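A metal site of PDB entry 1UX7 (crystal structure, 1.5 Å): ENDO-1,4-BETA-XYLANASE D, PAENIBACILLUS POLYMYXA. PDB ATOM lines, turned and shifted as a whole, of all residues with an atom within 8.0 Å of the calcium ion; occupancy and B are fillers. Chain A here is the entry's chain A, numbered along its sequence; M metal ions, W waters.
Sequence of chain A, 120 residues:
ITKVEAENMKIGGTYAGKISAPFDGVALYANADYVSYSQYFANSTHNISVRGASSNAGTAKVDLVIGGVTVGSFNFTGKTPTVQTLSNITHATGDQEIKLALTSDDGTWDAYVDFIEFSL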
ATOM      1  N   LYS A   3      33.981  28.511 -14.729  1.00  0.00           N
ATOM      2  CA  LYS A   3      32.935  27.775 -15.460  1.00  0.00           C
ATOM      3  C   LYS A   3      31.671  27.628 -14.636  1.00  0.00           C
ATOM      4  O   LYS A   3      31.705  27.129 -13.498  1.00  0.00           O
ATOM      5  CB  LYS A   3      33.441  26.373 -15.826  1.00  0.00           C
ATOM      6  CG  LYS A   3      32.486  25.550 -16.685  1.00  0.00           C
ATOM      7  CD  LYS A   3      33.137  24.191 -17.007  1.00  0.00           C
ATOM      8  CE  LYS A   3      32.288  23.381 -17.964  1.00  0.00           C
ATOM      9  NZ  LYS A   3      32.925  22.061 -18.259  1.00  0.00           N
ATOM     10  N   VAL A   4      30.539  28.037 -15.200  1.00  0.00           N
ATOM     11  CA  VAL A   4      29.250  27.935 -14.537  1.00  0.00           C
ATOM     12  C   VAL A   4      28.244  27.232 -15.418  1.00  0.00           C
ATOM     13  O   VAL A   4      27.970  27.656 -16.574  1.00  0.00           O
ATOM     14  CB  VAL A   4      28.725  29.337 -14.121  1.00  0.00           C
ATOM     15  CG1 VAL A   4      27.464  29.227 -13.304  1.00  0.00           C
ATOM     16  CG2 VAL A   4      29.802  30.123 -13.363  1.00  0.00           C
ATOM     17  N   GLU A   5      27.672  26.156 -14.895  1.00  0.00           N
ATOM     18  CA  GLU A   5      26.661  25.394 -15.631  1.00  0.00           C
ATOM     19  C   GLU A   5      25.324  26.118 -15.707  1.00  0.00           C
ATOM     20  O   GLU A   5      24.860  26.655 -14.707  1.00  0.00           O
ATOM     21  CB  GLU A   5      26.452  24.042 -14.978  1.00  0.00           C
ATOM     22  CG  GLU A   5      27.697  23.196 -14.891  1.00  0.00           C
ATOM     23  CD  GLU A   5      28.185  22.638 -16.213  1.00  0.00           C
ATOM     24  OE1 GLU A   5      27.408  22.594 -17.194  1.00  0.00           O
ATOM     25  OE2 GLU A   5      29.370  22.237 -16.268  1.00  0.00           O
ATOM     26  N   ALA A   6      24.701  26.158 -16.889  1.00  0.00           N
ATOM     27  CA  ALA A   6      23.433  26.834 -17.063  1.00  0.00           C
ATOM     28  C   ALA A   6      22.356  26.324 -16.097  1.00  0.00           C
ATOM     29  O   ALA A   6      21.546  27.083 -15.572  1.00  0.00           O
ATOM     30  CB  ALA A   6      22.953  26.731 -18.527  1.00  0.00           C
ATOM     31  N   GLU A   7      22.348  25.011 -15.908  1.00  0.00           N
ATOM     32  CA  GLU A   7      21.383  24.330 -15.056  1.00  0.00           C
ATOM     33  C   GLU A   7      21.470  24.727 -13.583  1.00  0.00           C
ATOM     34  O   GLU A   7      20.564  24.403 -12.822  1.00  0.00           O
ATOM     35  CB  GLU A   7      21.491  22.805 -15.259  1.00  0.00           C
ATOM     36  CG  GLU A   7      22.835  22.160 -14.915  1.00  0.00           C
ATOM     37  CD  GLU A   7      23.815  22.055 -16.076  1.00  0.00           C
ATOM     38  OE1 GLU A   7      23.747  22.933 -16.986  1.00  0.00           O
ATOM     39  OE2 GLU A   7      24.686  21.137 -16.086  1.00  0.00           O
ATOM     40  N   ASN A   8      22.554  25.388 -13.185  1.00  0.00           N
ATOM     41  CA  ASN A   8      22.734  25.869 -11.815  1.00  0.00           C
ATOM     42  C   ASN A   8      22.372  27.338 -11.629  1.00  0.00           C
ATOM     43  O   ASN A   8      22.399  27.863 -10.529  1.00  0.00           O
ATOM     44  CB  ASN A   8      24.171  25.587 -11.395  1.00  0.00           C
ATOM     45  CG  ASN A   8      24.471  24.066 -11.348  1.00  0.00           C
ATOM     46  OD1 ASN A   8      23.548  23.271 -11.253  1.00  0.00           O
ATOM     47  ND2 ASN A   8      25.693  23.718 -11.468  1.00  0.00           N
ATOM     48  N   ILE A  19      17.046  20.723 -19.320  1.00  0.00           N
ATOM     49  CA  ILE A  19      17.092  19.575 -20.217  1.00  0.00           C
ATOM     50  C   ILE A  19      18.233  18.629 -19.820  1.00  0.00           C
ATOM     51  O   ILE A  19      19.161  19.033 -19.142  1.00  0.00           O
ATOM     52  CB  ILE A  19      17.282  20.030 -21.692  1.00  0.00           C
ATOM     53  CG1 ILE A  19      18.553  20.869 -21.854  1.00  0.00           C
ATOM     54  CG2 ILE A  19      16.083  20.796 -22.180  1.00  0.00           C
ATOM     55  CD1 ILE A  19      18.797  21.324 -23.294  1.00  0.00           C
ATOM     56  N   PHE A  23      22.762  17.699 -23.576  1.00  0.00           N
ATOM     57  CA  PHE A  23      23.628  17.833 -22.427  1.00  0.00           C
ATOM     58  C   PHE A  23      22.717  18.198 -21.240  1.00  0.00           C
ATOM     59  O   PHE A  23      21.568  18.564 -21.426  1.00  0.00           O
ATOM     60  CB  PHE A  23      24.722  18.903 -22.623  1.00  0.00           C
ATOM     61  CG  PHE A  23      24.268  20.117 -23.437  1.00  0.00           C
ATOM     62  CD1 PHE A  23      23.289  20.961 -22.967  1.00  0.00           C
ATOM     63  CD2 PHE A  23      24.852  20.391 -24.655  1.00  0.00           C
ATOM     64  CE1 PHE A  23      22.852  22.039 -23.702  1.00  0.00           C
ATOM     65  CE2 PHE A  23      24.427  21.493 -25.403  1.00  0.00           C
ATOM     66  CZ  PHE A  23      23.434  22.307 -24.927  1.00  0.00           C
ATOM     67  N   ASP A  24      23.238  18.096 -20.030  1.00  0.00           N
ATOM     68  CA  ASP A  24      22.631  18.712 -18.873  1.00  0.00           C
ATOM     69  C   ASP A  24      22.731  20.233 -19.068  1.00  0.00           C
ATOM     70  O   ASP A  24      23.832  20.755 -19.205  1.00  0.00           O
ATOM     71  CB  ASP A  24      23.431  18.280 -17.635  1.00  0.00           C
ATOM     72  CG  ASP A  24      22.680  18.449 -16.354  1.00  0.00           C
ATOM     73  OD1 ASP A  24      21.679  19.181 -16.315  1.00  0.00           O
ATOM     74  OD2 ASP A  24      23.033  17.851 -15.309  1.00  0.00           O
ATOM     75  N   GLY A  25      21.593  20.896 -19.152  1.00  0.00           N
ATOM     76  CA  GLY A  25      21.580  22.336 -19.411  1.00  0.00           C
ATOM     77  C   GLY A  25      20.186  22.910 -19.335  1.00  0.00           C
ATOM     78  O   GLY A  25      19.317  22.381 -18.624  1.00  0.00           O
ATOM     79  N   VAL A  26      19.969  23.987 -20.087  1.00  0.00           N
ATOM     80  CA  VAL A  26      18.705  24.674 -20.100  1.00  0.00           C
ATOM     81  C   VAL A  26      18.310  25.026 -21.542  1.00  0.00           C
ATOM     82  O   VAL A  26      19.131  25.447 -22.348  1.00  0.00           O
ATOM     83  CB  VAL A  26      18.798  25.973 -19.246  1.00  0.00           C
ATOM     84  CG1 VAL A  26      17.529  26.818 -19.335  1.00  0.00           C
ATOM     85  CG2 VAL A  26      19.146  25.623 -17.786  1.00  0.00           C
ATOM     86  N   ARG A  51      29.038  26.629 -24.420  1.00  0.00           N
ATOM     87  CA  ARG A  51      28.684  25.407 -25.142  1.00  0.00           C
ATOM     88  C   ARG A  51      27.168  25.378 -25.263  1.00  0.00           C
ATOM     89  O   ARG A  51      26.455  25.626 -24.290  1.00  0.00           O
ATOM     90  CB  ARG A  51      29.206  24.159 -24.424  1.00  0.00           C
ATOM     91  CG  ARG A  51      28.997  22.890 -25.188  1.00  0.00           C
ATOM     92  CD  ARG A  51      29.842  21.735 -24.674  1.00  0.00           C
ATOM     93  NE  ARG A  51      29.811  20.532 -25.516  1.00  0.00           N
ATOM     94  CZ  ARG A  51      29.096  19.454 -25.279  1.00  0.00           C
ATOM     95  NH1 ARG A  51      28.269  19.388 -24.262  1.00  0.00           N
ATOM     96  NH2 ARG A  51      29.203  18.410 -26.098  1.00  0.00           N
ATOM     97  N   VAL A 113      21.498  25.541 -23.943  1.00  0.00           N
ATOM     98  CA  VAL A 113      22.698  26.111 -23.332  1.00  0.00           C
ATOM     99  C   VAL A 113      23.228  25.167 -22.243  1.00  0.00           C
ATOM    100  O   VAL A 113      22.482  24.746 -21.382  1.00  0.00           O
ATOM    101  CB  VAL A 113      22.392  27.513 -22.744  1.00  0.00           C
ATOM    102  CG1 VAL A 113      23.627  28.118 -22.166  1.00  0.00           C
ATOM    103  CG2 VAL A 113      21.810  28.432 -23.830  1.00  0.00           C
ATOM    104  N   ASP A 114      24.529  24.856 -22.316  1.00  0.00           N
ATOM    105  CA  ASP A 114      25.175  23.867 -21.447  1.00  0.00           C
ATOM    106  C   ASP A 114      25.908  24.543 -20.273  1.00  0.00           C
ATOM    107  O   ASP A 114      25.654  24.231 -19.110  1.00  0.00           O
ATOM    108  CB  ASP A 114      26.109  23.033 -22.313  1.00  0.00           C
ATOM    109  CG  ASP A 114      26.785  21.927 -21.590  1.00  0.00           C
ATOM    110  OD1 ASP A 114      26.500  21.716 -20.395  1.00  0.00           O
ATOM    111  OD2 ASP A 114      27.647  21.235 -22.172  1.00  0.00           O
ATOM    112  N   PHE A 115      26.794  25.495 -20.588  1.00  0.00           N
ATOM    113  CA  PHE A 115      27.596  26.211 -19.595  1.00  0.00           C
ATOM    114  C   PHE A 115      28.200  27.453 -20.246  1.00  0.00           C
ATOM    115  O   PHE A 115      28.221  27.583 -21.486  1.00  0.00           O
ATOM    116  CB  PHE A 115      28.722  25.336 -19.016  1.00  0.00           C
ATOM    117  CG  PHE A 115      29.744  24.832 -20.014  1.00  0.00           C
ATOM    118  CD1 PHE A 115      30.753  25.661 -20.493  1.00  0.00           C
ATOM    119  CD2 PHE A 115      29.724  23.490 -20.426  1.00  0.00           C
ATOM    120  CE1 PHE A 115      31.700  25.191 -21.408  1.00  0.00           C
ATOM    121  CE2 PHE A 115      30.718  23.021 -21.318  1.00  0.00           C
ATOM    122  CZ  PHE A 115      31.661  23.875 -21.808  1.00  0.00           C
ATOM    123  N   ILE A 116      28.693  28.328 -19.379  1.00  0.00           N
ATOM    124  CA  ILE A 116      29.509  29.472 -19.749  1.00  0.00           C
ATOM    125  C   ILE A 116      30.890  29.365 -19.069  1.00  0.00           C
ATOM    126  O   ILE A 116      30.977  28.892 -17.934  1.00  0.00           O
ATOM    127  CB  ILE A 116      28.805  30.808 -19.384  1.00  0.00           C
ATOM    128  CG1 ILE A 116      29.549  32.001 -20.002  1.00  0.00           C
ATOM    129  CG2 ILE A 116      28.613  31.005 -17.867  1.00  0.00           C
ATOM    130  CD1 ILE A 116      28.739  33.274 -20.123  1.00  0.00           C
HETATM  131 CA    CA M   1      25.645  21.849 -18.276  1.00  0.00          CA
HETATM  132  O   HOH W   1      26.699  19.701 -18.125  1.00  0.00           O
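The calcium ion is bound by OE1 of Glu 5 (2.2 Å), OD1 of Asp 114 (2.3 Å), O of Asp 24 (2.3 Å), water W1 (2.4 Å), OE2 of Glu 7 (2.5 Å), O of Asp 114 (2.5 Å) and OE1 of Glu 7 (2.5 Å).
N of Ala 6 sits close to O of Asp 114 (3.1 Å).
The guanidinium group (NH1) of Arg 51 is in salt-bridge range of the side-chain carboxylate (OD2) of Asp 114 (2.9 Å).
Of the 16 residues printed, 4 come within 4 Å of the calcium ion.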
